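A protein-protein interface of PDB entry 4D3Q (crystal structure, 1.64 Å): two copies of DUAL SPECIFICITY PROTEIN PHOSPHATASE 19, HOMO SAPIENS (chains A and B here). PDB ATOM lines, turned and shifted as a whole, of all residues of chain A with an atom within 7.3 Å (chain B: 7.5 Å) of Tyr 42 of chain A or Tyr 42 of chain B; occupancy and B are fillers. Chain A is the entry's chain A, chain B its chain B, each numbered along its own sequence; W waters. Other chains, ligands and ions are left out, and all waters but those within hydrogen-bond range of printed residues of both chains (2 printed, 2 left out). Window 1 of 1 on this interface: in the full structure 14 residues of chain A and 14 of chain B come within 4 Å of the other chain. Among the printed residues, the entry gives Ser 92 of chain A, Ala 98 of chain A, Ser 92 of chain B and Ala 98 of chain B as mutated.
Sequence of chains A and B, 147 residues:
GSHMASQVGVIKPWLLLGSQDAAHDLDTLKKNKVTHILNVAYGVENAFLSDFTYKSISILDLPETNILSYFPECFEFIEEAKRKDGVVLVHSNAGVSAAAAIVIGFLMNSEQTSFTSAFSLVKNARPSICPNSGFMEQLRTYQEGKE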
ATOM      1  N   GLN A  20     -14.143 -33.288 -17.031  1.00  0.00           N
ATOM      2  CA  GLN A  20     -15.362 -32.756 -17.563  1.00  0.00           C
ATOM      3  C   GLN A  20     -16.259 -33.772 -18.234  1.00  0.00           C
ATOM      4  O   GLN A  20     -17.458 -33.625 -18.168  1.00  0.00           O
ATOM      5  CB  GLN A  20     -15.089 -31.594 -18.530  1.00  0.00           C
ATOM      6  CG  GLN A  20     -14.292 -31.958 -19.747  1.00  0.00           C
ATOM      7  CD  GLN A  20     -13.759 -30.792 -20.503  1.00  0.00           C
ATOM      8  OE1 GLN A  20     -12.520 -30.718 -20.804  1.00  0.00           O
ATOM      9  NE2 GLN A  20     -14.601 -29.875 -20.795  1.00  0.00           N
ATOM     10  N   ASN A  39     -17.710 -28.428  -9.363  1.00  0.00           N
ATOM     11  CA  ASN A  39     -17.159 -28.043 -10.656  1.00  0.00           C
ATOM     12  C   ASN A  39     -16.121 -26.923 -10.539  1.00  0.00           C
ATOM     13  O   ASN A  39     -16.477 -25.783 -10.287  1.00  0.00           O
ATOM     14  CB  ASN A  39     -18.331 -27.581 -11.517  1.00  0.00           C
ATOM     15  CG  ASN A  39     -17.945 -27.155 -12.898  1.00  0.00           C
ATOM     16  OD1 ASN A  39     -16.790 -26.951 -13.238  1.00  0.00           O
ATOM     17  ND2 ASN A  39     -18.977 -26.934 -13.748  1.00  0.00           N
ATOM     18  N   VAL A  40     -14.851 -27.288 -10.607  1.00  0.00           N
ATOM     19  CA  VAL A  40     -13.787 -26.294 -10.500  1.00  0.00           C
ATOM     20  C   VAL A  40     -13.135 -25.958 -11.880  1.00  0.00           C
ATOM     21  O   VAL A  40     -12.099 -25.250 -11.933  1.00  0.00           O
ATOM     22  CB  VAL A  40     -12.722 -26.696  -9.422  1.00  0.00           C
ATOM     23  CG1 VAL A  40     -13.442 -27.087  -8.143  1.00  0.00           C
ATOM     24  CG2 VAL A  40     -11.729 -27.813  -9.869  1.00  0.00           C
ATOM     25  N   ALA A  41     -13.820 -26.364 -12.972  1.00  0.00           N
ATOM     26  CA  ALA A  41     -13.383 -26.128 -14.307  1.00  0.00           C
ATOM     27  C   ALA A  41     -13.630 -24.710 -14.819  1.00  0.00           C
ATOM     28  O   ALA A  41     -14.286 -23.902 -14.141  1.00  0.00           O
ATOM     29  CB  ALA A  41     -14.119 -27.111 -15.252  1.00  0.00           C
ATOM     30  N   TYR A  42     -13.104 -24.443 -16.010  1.00  0.00           N
ATOM     31  CA  TYR A  42     -13.628 -23.307 -16.799  1.00  0.00           C
ATOM     32  C   TYR A  42     -14.524 -23.820 -17.840  1.00  0.00           C
ATOM     33  O   TYR A  42     -14.276 -24.836 -18.514  1.00  0.00           O
ATOM     34  CB  TYR A  42     -12.517 -22.420 -17.426  1.00  0.00           C
ATOM     35  CG  TYR A  42     -11.534 -23.176 -18.280  1.00  0.00           C
ATOM     36  CD1 TYR A  42     -11.786 -23.370 -19.665  1.00  0.00           C
ATOM     37  CD2 TYR A  42     -10.346 -23.741 -17.749  1.00  0.00           C
ATOM     38  CE1 TYR A  42     -10.893 -24.079 -20.457  1.00  0.00           C
ATOM     39  CE2 TYR A  42      -9.438 -24.408 -18.604  1.00  0.00           C
ATOM     40  CZ  TYR A  42      -9.732 -24.605 -19.943  1.00  0.00           C
ATOM     41  OH  TYR A  42      -8.833 -25.266 -20.740  1.00  0.00           O
ATOM     42  N   GLY A  43     -15.615 -23.122 -18.047  1.00  0.00           N
ATOM     43  CA  GLY A  43     -16.476 -23.375 -19.224  1.00  0.00           C
ATOM     44  C   GLY A  43     -17.310 -24.613 -19.312  1.00  0.00           C
ATOM     45  O   GLY A  43     -17.867 -24.903 -20.407  1.00  0.00           O
ATOM     46  N   VAL A  44     -17.439 -25.375 -18.205  1.00  0.00           N
ATOM     47  CA  VAL A  44     -18.161 -26.639 -18.214  1.00  0.00           C
ATOM     48  C   VAL A  44     -19.526 -26.450 -17.628  1.00  0.00           C
ATOM     49  O   VAL A  44     -19.711 -26.156 -16.428  1.00  0.00           O
ATOM     50  CB  VAL A  44     -17.411 -27.759 -17.439  1.00  0.00           C
ATOM     51  CG1 VAL A  44     -18.217 -29.037 -17.388  1.00  0.00           C
ATOM     52  CG2 VAL A  44     -16.019 -27.975 -18.032  1.00  0.00           C
ATOM     53  N   GLU A  45     -20.564 -26.521 -18.490  1.00  0.00           N
ATOM     54  CA  GLU A  45     -21.918 -26.337 -18.039  1.00  0.00           C
ATOM     55  C   GLU A  45     -22.376 -27.435 -17.020  1.00  0.00           C
ATOM     56  O   GLU A  45     -22.006 -28.622 -17.214  1.00  0.00           O
ATOM     57  CB  GLU A  45     -22.918 -26.343 -19.237  1.00  0.00           C
ATOM     58  CG  GLU A  45     -22.752 -25.199 -20.195  1.00  0.00           C
ATOM     59  CD  GLU A  45     -23.669 -25.212 -21.407  1.00  0.00           C
ATOM     60  OE1 GLU A  45     -24.694 -25.925 -21.355  1.00  0.00           O
ATOM     61  OE2 GLU A  45     -23.283 -24.431 -22.330  1.00  0.00           O
ATOM     62  N   ILE A  57     -16.590 -23.401  -8.446  1.00  0.00           N
ATOM     63  CA  ILE A  57     -15.539 -22.536  -7.917  1.00  0.00           C
ATOM     64  C   ILE A  57     -14.383 -22.589  -8.916  1.00  0.00           C
ATOM     65  O   ILE A  57     -13.931 -23.671  -9.245  1.00  0.00           O
ATOM     66  CB  ILE A  57     -15.007 -22.904  -6.512  1.00  0.00           C
ATOM     67  CG1 ILE A  57     -16.000 -22.956  -5.362  1.00  0.00           C
ATOM     68  CG2 ILE A  57     -14.021 -21.822  -6.075  1.00  0.00           C
ATOM     69  CD1 ILE A  57     -16.279 -21.553  -4.737  1.00  0.00           C
ATOM     70  N   SER A  58     -13.914 -21.417  -9.433  1.00  0.00           N
ATOM     71  CA  SER A  58     -12.847 -21.433 -10.437  1.00  0.00           C
ATOM     72  C   SER A  58     -11.476 -21.658  -9.896  1.00  0.00           C
ATOM     73  O   SER A  58     -10.995 -20.848  -9.099  1.00  0.00           O
ATOM     74  CB  SER A  58     -12.906 -20.083 -11.127  1.00  0.00           C
ATOM     75  OG  SER A  58     -11.844 -19.942 -12.077  1.00  0.00           O
ATOM     76  N   ILE A  59     -10.868 -22.803 -10.309  1.00  0.00           N
ATOM     77  CA  ILE A  59      -9.515 -23.117  -9.804  1.00  0.00           C
ATOM     78  C   ILE A  59      -8.634 -23.416 -10.967  1.00  0.00           C
ATOM     79  O   ILE A  59      -8.601 -24.566 -11.460  1.00  0.00           O
ATOM     80  CB  ILE A  59      -9.564 -24.273  -8.792  1.00  0.00           C
ATOM     81  CG1 ILE A  59     -10.515 -23.991  -7.666  1.00  0.00           C
ATOM     82  CG2 ILE A  59      -8.129 -24.415  -8.278  1.00  0.00           C
ATOM     83  CD1 ILE A  59     -10.495 -25.052  -6.595  1.00  0.00           C
ATOM     84  N   LEU A  60      -7.937 -22.391 -11.428  1.00  0.00           N
ATOM     85  CA  LEU A  60      -7.072 -22.522 -12.607  1.00  0.00           C
ATOM     86  C   LEU A  60      -5.834 -23.336 -12.342  1.00  0.00           C
ATOM     87  O   LEU A  60      -5.302 -23.312 -11.230  1.00  0.00           O
ATOM     88  CB  LEU A  60      -6.690 -21.142 -13.083  1.00  0.00           C
ATOM     89  CG  LEU A  60      -7.822 -20.245 -13.667  1.00  0.00           C
ATOM     90  CD1 LEU A  60      -7.236 -18.902 -14.048  1.00  0.00           C
ATOM     91  CD2 LEU A  60      -8.549 -20.891 -14.802  1.00  0.00           C
ATOM     92  N   ASP A  61      -5.429 -24.088 -13.351  1.00  0.00           N
ATOM     93  CA  ASP A  61      -4.282 -25.022 -13.236  1.00  0.00           C
ATOM     94  C   ASP A  61      -2.984 -24.235 -13.502  1.00  0.00           C
ATOM     95  O   ASP A  61      -2.400 -24.364 -14.560  1.00  0.00           O
ATOM     96  CB  ASP A  61      -4.392 -26.203 -14.132  1.00  0.00           C
ATOM     97  CG  ASP A  61      -3.215 -27.159 -13.951  1.00  0.00           C
ATOM     98  OD1 ASP A  61      -2.556 -27.048 -12.900  1.00  0.00           O
ATOM     99  OD2 ASP A  61      -3.022 -27.990 -14.870  1.00  0.00           O
ATOM    100  N   LEU A  62      -2.542 -23.405 -12.570  1.00  0.00           N
ATOM    101  CA  LEU A  62      -1.338 -22.601 -12.626  1.00  0.00           C
ATOM    102  C   LEU A  62      -0.684 -22.670 -11.236  1.00  0.00           C
ATOM    103  O   LEU A  62      -1.368 -22.747 -10.157  1.00  0.00           O
ATOM    104  CB  LEU A  62      -1.718 -21.128 -12.911  1.00  0.00           C
ATOM    105  CG  LEU A  62      -2.363 -20.850 -14.277  1.00  0.00           C
ATOM    106  CD1 LEU A  62      -3.027 -19.444 -14.262  1.00  0.00           C
ATOM    107  CD2 LEU A  62      -1.342 -21.015 -15.324  1.00  0.00           C
ATOM    108  N   THR A  65      -1.935 -20.099  -8.810  1.00  0.00           N
ATOM    109  CA  THR A  65      -3.188 -20.264  -8.130  1.00  0.00           C
ATOM    110  C   THR A  65      -2.947 -20.651  -6.682  1.00  0.00           C
ATOM    111  O   THR A  65      -2.174 -21.587  -6.439  1.00  0.00           O
ATOM    112  CB  THR A  65      -3.997 -21.348  -8.841  1.00  0.00           C
ATOM    113  OG1 THR A  65      -4.344 -20.884 -10.155  1.00  0.00           O
ATOM    114  CG2 THR A  65      -5.272 -21.749  -8.154  1.00  0.00           C
ATOM    115  N   HIS A  91     -14.713 -32.368 -10.113  1.00  0.00           N
ATOM    116  CA  HIS A  91     -14.196 -32.449 -11.438  1.00  0.00           C
ATOM    117  C   HIS A  91     -13.669 -31.068 -11.891  1.00  0.00           C
ATOM    118  O   HIS A  91     -13.965 -30.048 -11.322  1.00  0.00           O
ATOM    119  CB  HIS A  91     -15.219 -32.888 -12.480  1.00  0.00           C
ATOM    120  CG  HIS A  91     -16.184 -31.818 -12.916  1.00  0.00           C
ATOM    121  ND1 HIS A  91     -15.889 -30.954 -13.966  1.00  0.00           N
ATOM    122  CD2 HIS A  91     -17.421 -31.439 -12.453  1.00  0.00           C
ATOM    123  CE1 HIS A  91     -16.930 -30.168 -14.170  1.00  0.00           C
ATOM    124  NE2 HIS A  91     -17.864 -30.422 -13.264  1.00  0.00           N
ATOM    125  N   SER A  92     -12.819 -31.088 -12.923  1.00  0.00           N
ATOM    126  CA  SER A  92     -12.375 -29.865 -13.574  1.00  0.00           C
ATOM    127  C   SER A  92     -12.447 -30.117 -15.096  1.00  0.00           C
ATOM    128  O   SER A  92     -13.490 -30.644 -15.571  1.00  0.00           O
ATOM    129  CB  SER A  92     -11.075 -29.345 -13.033  1.00  0.00           C
ATOM    130  OG  SER A  92     -10.825 -28.028 -13.614  1.00  0.00           O
ATOM    131  N   ASN A  93     -11.489 -29.615 -15.844  1.00  0.00           N
ATOM    132  CA  ASN A  93     -11.408 -29.851 -17.242  1.00  0.00           C
ATOM    133  C   ASN A  93     -10.786 -31.224 -17.405  1.00  0.00           C
ATOM    134  O   ASN A  93     -11.481 -32.212 -17.467  1.00  0.00           O
ATOM    135  CB  ASN A  93     -10.708 -28.683 -17.978  1.00  0.00           C
ATOM    136  CG  ASN A  93     -11.520 -27.411 -17.917  1.00  0.00           C
ATOM    137  OD1 ASN A  93     -11.478 -26.738 -16.889  1.00  0.00           O
ATOM    138  ND2 ASN A  93     -12.275 -27.104 -18.977  1.00  0.00           N
ATOM    139  N   ALA A  94      -9.470 -31.291 -17.462  1.00  0.00           N
ATOM    140  CA  ALA A  94      -8.845 -32.634 -17.487  1.00  0.00           C
ATOM    141  C   ALA A  94      -8.982 -33.369 -16.129  1.00  0.00           C
ATOM    142  O   ALA A  94      -8.967 -34.587 -16.047  1.00  0.00           O
ATOM    143  CB  ALA A  94      -7.386 -32.483 -17.838  1.00  0.00           C
ATOM    144  N   ALA A  98      -5.680 -29.321 -10.631  1.00  0.00           N
ATOM    145  CA  ALA A  98      -6.412 -28.564  -9.634  1.00  0.00           C
ATOM    146  C   ALA A  98      -7.439 -29.410  -8.931  1.00  0.00           C
ATOM    147  O   ALA A  98      -7.572 -29.357  -7.711  1.00  0.00           O
ATOM    148  CB  ALA A  98      -7.084 -27.326 -10.181  1.00  0.00           C
ATOM    149  N   GLN B  20       3.269 -27.586 -18.165  1.00  0.00           N
ATOM    150  CA  GLN B  20       3.897 -26.300 -17.865  1.00  0.00           C
ATOM    151  C   GLN B  20       5.163 -26.371 -17.018  1.00  0.00           C
ATOM    152  O   GLN B  20       6.028 -25.461 -17.143  1.00  0.00           O
ATOM    153  CB  GLN B  20       2.822 -25.412 -17.172  1.00  0.00           C
ATOM    154  CG  GLN B  20       2.420 -25.902 -15.796  1.00  0.00           C
ATOM    155  CD  GLN B  20       1.168 -25.233 -15.297  1.00  0.00           C
ATOM    156  OE1 GLN B  20       0.131 -25.865 -14.946  1.00  0.00           O
ATOM    157  NE2 GLN B  20       1.233 -24.005 -15.323  1.00  0.00           N
ATOM    158  N   ASN B  39       3.642 -23.454 -27.136  1.00  0.00           N
ATOM    159  CA  ASN B  39       2.925 -23.230 -25.866  1.00  0.00           C
ATOM    160  C   ASN B  39       1.465 -23.066 -26.184  1.00  0.00           C
ATOM    161  O   ASN B  39       1.024 -22.039 -26.702  1.00  0.00           O
ATOM    162  CB  ASN B  39       3.476 -21.953 -25.252  1.00  0.00           C
ATOM    163  CG  ASN B  39       2.791 -21.591 -23.961  1.00  0.00           C
ATOM    164  OD1 ASN B  39       1.714 -22.139 -23.602  1.00  0.00           O
ATOM    165  ND2 ASN B  39       3.355 -20.596 -23.228  1.00  0.00           N
ATOM    166  N   VAL B  40       0.699 -24.113 -25.909  1.00  0.00           N
ATOM    167  CA  VAL B  40      -0.755 -24.181 -26.115  1.00  0.00           C
ATOM    168  C   VAL B  40      -1.452 -24.166 -24.744  1.00  0.00           C
ATOM    169  O   VAL B  40      -2.675 -24.430 -24.659  1.00  0.00           O
ATOM    170  CB  VAL B  40      -1.324 -25.216 -27.076  1.00  0.00           C
ATOM    171  CG1 VAL B  40      -0.642 -25.059 -28.447  1.00  0.00           C
ATOM    172  CG2 VAL B  40      -1.162 -26.631 -26.505  1.00  0.00           C
ATOM    173  N   ALA B  41      -0.732 -23.732 -23.718  1.00  0.00           N
ATOM    174  CA  ALA B  41      -1.259 -23.501 -22.347  1.00  0.00           C
ATOM    175  C   ALA B  41      -1.905 -22.134 -22.280  1.00  0.00           C
ATOM    176  O   ALA B  41      -1.891 -21.339 -23.231  1.00  0.00           O
ATOM    177  CB  ALA B  41      -0.151 -23.587 -21.332  1.00  0.00           C
ATOM    178  N   TYR B  42      -2.579 -21.977 -21.141  1.00  0.00           N
ATOM    179  CA  TYR B  42      -2.970 -20.577 -20.703  1.00  0.00           C
ATOM    180  C   TYR B  42      -2.118 -20.209 -19.568  1.00  0.00           C
ATOM    181  O   TYR B  42      -1.819 -20.965 -18.685  1.00  0.00           O
ATOM    182  CB  TYR B  42      -4.448 -20.499 -20.371  1.00  0.00           C
ATOM    183  CG  TYR B  42      -4.885 -21.368 -19.254  1.00  0.00           C
ATOM    184  CD1 TYR B  42      -4.862 -20.971 -17.922  1.00  0.00           C
ATOM    185  CD2 TYR B  42      -5.416 -22.660 -19.513  1.00  0.00           C
ATOM    186  CE1 TYR B  42      -5.221 -21.755 -16.881  1.00  0.00           C
ATOM    187  CE2 TYR B  42      -5.766 -23.491 -18.462  1.00  0.00           C
ATOM    188  CZ  TYR B  42      -5.681 -23.053 -17.131  1.00  0.00           C
ATOM    189  OH  TYR B  42      -6.093 -23.978 -16.182  1.00  0.00           O
ATOM    190  N   GLY B  43      -1.747 -18.918 -19.526  1.00  0.00           N
ATOM    191  CA  GLY B  43      -1.054 -18.370 -18.353  1.00  0.00           C
ATOM    192  C   GLY B  43       0.323 -18.763 -18.030  1.00  0.00           C
ATOM    193  O   GLY B  43       0.840 -18.466 -16.962  1.00  0.00           O
ATOM    194  N   VAL B  44       0.971 -19.463 -19.002  1.00  0.00           N
ATOM    195  CA  VAL B  44       2.382 -19.958 -18.829  1.00  0.00           C
ATOM    196  C   VAL B  44       3.356 -19.062 -19.535  1.00  0.00           C
ATOM    197  O   VAL B  44       3.386 -19.065 -20.754  1.00  0.00           O
ATOM    198  CB  VAL B  44       2.542 -21.436 -19.283  1.00  0.00           C
ATOM    199  CG1 VAL B  44       3.956 -21.956 -19.085  1.00  0.00           C
ATOM    200  CG2 VAL B  44       1.545 -22.285 -18.538  1.00  0.00           C
ATOM    201  N   GLU B  45       4.162 -18.307 -18.788  1.00  0.00           N
ATOM    202  CA  GLU B  45       5.110 -17.363 -19.406  1.00  0.00           C
ATOM    203  C   GLU B  45       6.170 -18.166 -20.204  1.00  0.00           C
ATOM    204  O   GLU B  45       6.584 -19.186 -19.686  1.00  0.00           O
ATOM    205  CB  GLU B  45       5.760 -16.521 -18.373  1.00  0.00           C
ATOM    206  CG  GLU B  45       4.808 -15.552 -17.661  1.00  0.00           C
ATOM    207  CD  GLU B  45       5.425 -14.704 -16.594  1.00  0.00           C
ATOM    208  OE1 GLU B  45       6.664 -14.641 -16.428  1.00  0.00           O
ATOM    209  OE2 GLU B  45       4.642 -14.029 -15.813  1.00  0.00           O
ATOM    210  N   ILE B  57      -0.333 -20.542 -29.043  1.00  0.00           N
ATOM    211  CA  ILE B  57      -1.645 -20.627 -29.623  1.00  0.00           C
ATOM    212  C   ILE B  57      -2.602 -20.935 -28.464  1.00  0.00           C
ATOM    213  O   ILE B  57      -2.342 -21.859 -27.713  1.00  0.00           O
ATOM    214  CB  ILE B  57      -1.739 -21.713 -30.741  1.00  0.00           C
ATOM    215  CG1 ILE B  57      -0.827 -21.335 -31.911  1.00  0.00           C
ATOM    216  CG2 ILE B  57      -3.166 -21.863 -31.209  1.00  0.00           C
ATOM    217  CD1 ILE B  57      -1.362 -20.207 -32.786  1.00  0.00           C
ATOM    218  N   SER B  58      -3.690 -20.189 -28.306  1.00  0.00           N
ATOM    219  CA  SER B  58      -4.736 -20.573 -27.258  1.00  0.00           C
ATOM    220  C   SER B  58      -5.617 -21.650 -27.644  1.00  0.00           C
ATOM    221  O   SER B  58      -6.333 -21.571 -28.704  1.00  0.00           O
ATOM    222  CB  SER B  58      -5.654 -19.335 -26.924  1.00  0.00           C
ATOM    223  OG  SER B  58      -6.694 -19.606 -26.008  1.00  0.00           O
ATOM    224  N   ILE B  59      -5.562 -22.785 -26.851  1.00  0.00           N
ATOM    225  CA  ILE B  59      -6.431 -23.888 -27.150  1.00  0.00           C
ATOM    226  C   ILE B  59      -7.167 -24.301 -25.880  1.00  0.00           C
ATOM    227  O   ILE B  59      -6.569 -24.999 -25.026  1.00  0.00           O
ATOM    228  CB  ILE B  59      -5.709 -25.094 -27.748  1.00  0.00           C
ATOM    229  CG1 ILE B  59      -4.858 -24.625 -28.933  1.00  0.00           C
ATOM    230  CG2 ILE B  59      -6.759 -26.160 -28.119  1.00  0.00           C
ATOM    231  CD1 ILE B  59      -4.210 -25.764 -29.661  1.00  0.00           C
ATOM    232  N   LEU B  60      -8.420 -23.872 -25.758  1.00  0.00           N
ATOM    233  CA  LEU B  60      -9.232 -24.208 -24.545  1.00  0.00           C
ATOM    234  C   LEU B  60      -9.525 -25.699 -24.497  1.00  0.00           C
ATOM    235  O   LEU B  60      -9.960 -26.263 -25.510  1.00  0.00           O
ATOM    236  CB  LEU B  60     -10.469 -23.378 -24.418  1.00  0.00           C
ATOM    237  CG  LEU B  60     -10.237 -21.867 -24.191  1.00  0.00           C
ATOM    238  CD1 LEU B  60     -11.590 -21.237 -24.070  1.00  0.00           C
ATOM    239  CD2 LEU B  60      -9.373 -21.618 -22.984  1.00  0.00           C
ATOM    240  N   ASP B  61      -9.389 -26.330 -23.336  1.00  0.00           N
ATOM    241  CA  ASP B  61      -9.720 -27.761 -23.209  1.00  0.00           C
ATOM    242  C   ASP B  61     -11.170 -27.914 -22.960  1.00  0.00           C
ATOM    243  O   ASP B  61     -11.614 -28.167 -21.806  1.00  0.00           O
ATOM    244  CB  ASP B  61      -8.927 -28.378 -22.060  1.00  0.00           C
ATOM    245  CG  ASP B  61      -9.198 -29.859 -21.896  1.00  0.00           C
ATOM    246  OD1 ASP B  61      -9.564 -30.429 -22.999  1.00  0.00           O
ATOM    247  OD2 ASP B  61      -8.970 -30.432 -20.844  1.00  0.00           O
ATOM    248  N   LEU B  62     -12.026 -27.806 -24.016  1.00  0.00           N
ATOM    249  CA  LEU B  62     -13.470 -27.973 -23.935  1.00  0.00           C
ATOM    250  C   LEU B  62     -13.832 -28.794 -25.185  1.00  0.00           C
ATOM    251  O   LEU B  62     -13.183 -28.632 -26.242  1.00  0.00           O
ATOM    252  CB  LEU B  62     -14.151 -26.631 -24.046  1.00  0.00           C
ATOM    253  CG  LEU B  62     -13.950 -25.727 -22.814  1.00  0.00           C
ATOM    254  CD1 LEU B  62     -14.471 -24.325 -23.077  1.00  0.00           C
ATOM    255  CD2 LEU B  62     -14.639 -26.288 -21.653  1.00  0.00           C
ATOM    256  N   THR B  65     -14.291 -26.767 -28.438  1.00  0.00           N
ATOM    257  CA  THR B  65     -13.112 -26.269 -29.115  1.00  0.00           C
ATOM    258  C   THR B  65     -12.935 -27.045 -30.388  1.00  0.00           C
ATOM    259  O   THR B  65     -12.943 -28.276 -30.319  1.00  0.00           O
ATOM    260  CB  THR B  65     -11.891 -26.353 -28.238  1.00  0.00           C
ATOM    261  OG1 THR B  65     -12.140 -25.464 -27.101  1.00  0.00           O
ATOM    262  CG2 THR B  65     -10.615 -25.960 -28.916  1.00  0.00           C
ATOM    263  N   HIS B  91       3.536 -28.149 -25.239  1.00  0.00           N
ATOM    264  CA  HIS B  91       3.101 -28.211 -23.878  1.00  0.00           C
ATOM    265  C   HIS B  91       1.781 -27.424 -23.736  1.00  0.00           C
ATOM    266  O   HIS B  91       1.538 -26.505 -24.474  1.00  0.00           O
ATOM    267  CB  HIS B  91       4.131 -27.741 -22.837  1.00  0.00           C
ATOM    268  CG  HIS B  91       4.218 -26.249 -22.715  1.00  0.00           C
ATOM    269  ND1 HIS B  91       3.349 -25.573 -21.901  1.00  0.00           N
ATOM    270  CD2 HIS B  91       5.052 -25.339 -23.273  1.00  0.00           C
ATOM    271  CE1 HIS B  91       3.697 -24.263 -21.944  1.00  0.00           C
ATOM    272  NE2 HIS B  91       4.660 -24.086 -22.826  1.00  0.00           N
ATOM    273  N   SER B  92       1.043 -27.876 -22.745  1.00  0.00           N
ATOM    274  CA  SER B  92      -0.156 -27.119 -22.263  1.00  0.00           C
ATOM    275  C   SER B  92       0.051 -26.937 -20.755  1.00  0.00           C
ATOM    276  O   SER B  92       1.176 -26.644 -20.273  1.00  0.00           O
ATOM    277  CB  SER B  92      -1.414 -27.731 -22.751  1.00  0.00           C
ATOM    278  OG  SER B  92      -1.572 -29.125 -22.346  1.00  0.00           O
ATOM    279  N   ASN B  93      -1.081 -26.930 -19.988  1.00  0.00           N
ATOM    280  CA  ASN B  93      -0.940 -26.740 -18.557  1.00  0.00           C
ATOM    281  C   ASN B  93      -0.497 -28.062 -17.940  1.00  0.00           C
ATOM    282  O   ASN B  93       0.588 -28.145 -17.464  1.00  0.00           O
ATOM    283  CB  ASN B  93      -2.256 -26.150 -18.023  1.00  0.00           C
ATOM    284  CG  ASN B  93      -2.453 -24.698 -18.445  1.00  0.00           C
ATOM    285  OD1 ASN B  93      -2.640 -24.435 -19.600  1.00  0.00           O
ATOM    286  ND2 ASN B  93      -2.223 -23.787 -17.517  1.00  0.00           N
ATOM    287  N   ALA B  94      -1.359 -29.068 -18.006  1.00  0.00           N
ATOM    288  CA  ALA B  94      -1.032 -30.460 -17.558  1.00  0.00           C
ATOM    289  C   ALA B  94      -0.421 -31.291 -18.693  1.00  0.00           C
ATOM    290  O   ALA B  94       0.279 -32.302 -18.445  1.00  0.00           O
ATOM    291  CB  ALA B  94      -2.185 -31.125 -16.981  1.00  0.00           C
ATOM    292  N   ALA B  98      -5.294 -30.782 -24.598  1.00  0.00           N
ATOM    293  CA  ALA B  98      -5.159 -30.210 -25.934  1.00  0.00           C
ATOM    294  C   ALA B  98      -3.766 -30.393 -26.567  1.00  0.00           C
ATOM    295  O   ALA B  98      -3.695 -30.583 -27.794  1.00  0.00           O
ATOM    296  CB  ALA B  98      -5.529 -28.728 -26.027  1.00  0.00           C
HETATM  297  O   HOH W   1      -7.614 -29.283 -18.905  1.00  0.00           O
HETATM  298  O   HOH W   2      -6.181 -24.415 -22.454  1.00  0.00           O
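Gln 20 of chain A touches Leu 62 of chain B, and with the chains exchanged Leu 62 of chain A touches Gln 20 of chain B.
Tyr 42 of chain B touches its own counterpart, Tyr 42 of chain A.
Leu 62 of chain A touches Asn 93 of chain B, and with the chains exchanged Asn 93 of chain A touches Leu 62 of chain B.
The side-chain amide oxygen of Gln 20 of chain A sits close to the backbone carbonyl oxygen of Asp 61 of chain B (2.9 Å).
The backbone NH (N) of Asp 61 of chain B sits at hydrogen-bond distance from the side-chain hydroxyl (OH) of Tyr 42 of chain A, at 2.9 Å.
O of Asp 61 of chain A sits close to OE1 of Gln 20 of chain B, at 3.0 Å.
The backbone NH (N) of Asp 61 of chain A is in hydrogen-bond range of the side-chain hydroxyl (OH) of Tyr 42 of chain B, at 2.9 Å.
O of Asp 61 of chain A sits at hydrogen-bond distance from ND2 of Asn 93 of chain B.
O of Asp 61 of chain B lies within hydrogen-bond range of ND2 of Asn 93 of chain A (3.1 Å).
O of Ser 92 of chain A lies within hydrogen-bond range of N of Gln 20 of chain A (3.1 Å).
O of Leu 60 of chain A lies within hydrogen-bond range of OG1 of Thr 65 of chain A (2.8 Å).
The backbone carbonyl oxygen of Leu 60 of chain B sits at hydrogen-bond distance from the side-chain hydroxyl of Thr 65 of chain B (2.8 Å).
Water W1 lies within hydrogen-bond range of OD2 of Asp 61 of chain B (2.6 Å) and N of Ala 94 of chain A (3.1 Å).
Water W2 lies within hydrogen-bond range of O of Ile 59 of chain B (2.7 Å) and OH of Tyr 42 of chain A (3.3 Å).
Of the 20 printed residues of chain B, 8 touch a printed residue of chain A.
Hydrophobic or aromatic side chains of chain B within 4 Å of the printed part of chain A: Tyr 42, Leu 60, Leu 62 and Ala 94.
Along chain B the printed residues that touch a printed residue of chain A span positions 20 to 94.
Of the 20 printed residues of chain A, 8 touch a printed residue of chain B.
Along chain A the printed residues that touch a printed residue of chain B span positions 20 to 94.
Among the printed residues, 19 pairs touch across the chains.
Among the printed residues, no Asp or Glu carboxylate lies within 4 Å of a Lys or Arg side-chain nitrogen of the other chain.
Among the printed residues, pairs that only touch across the chains: Gln 20 of chain A with Leu 62 of chain B, Tyr 42 of chain A with Tyr 42 of chain B, Tyr 42 of chain A with Leu 60 of chain B, Tyr 42 of chain A with Leu 62 of chain B, Gly 43 of chain A with Leu 62 of chain B, Leu 60 of chain A with Tyr 42 of chain B, Asp 61 of chain A with Ala 94 of chain B, Leu 62 of chain A with Gln 20 of chain B, Leu 62 of chain A with Tyr 42 of chain B, Leu 62 of chain A with Gly 43 of chain B, Leu 62 of chain A with Asn 93 of chain B, Asn 93 of chain A with Leu 62 of chain B and Ala 94 of chain A with Asp 61 of chain B.
Of the printed residues of chain B, Leu 60 of chain A touches Tyr 42.
Printed residues of chain B within 4 Å of Asn 93 of chain A: Asp 61 and Leu 62.
Of the printed residues of chain B, Ala 94 of chain A touches Asp 61.
Tyr 42 of chain B touches just these residues of chain A: Tyr 42 (3.8 Å), Leu 60 (3.9 Å), Asp 61 (2.9 Å) and Leu 62 (3.4 Å).
Printed residues of chain A within 4 Å of Asp 61 of chain B: Gln 20 (2.9 Å), Tyr 42 (2.9 Å), Asn 93 (3.1 Å) and Ala 94 (3.5 Å).
The nearest residue of chain B that does not touch Tyr 42 of chain A is Ile 59 of chain B (4.9 Å).
The nearest printed residue of chain A that does not touch Leu 62 of chain B is Val 44 of chain A (4.2 Å).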
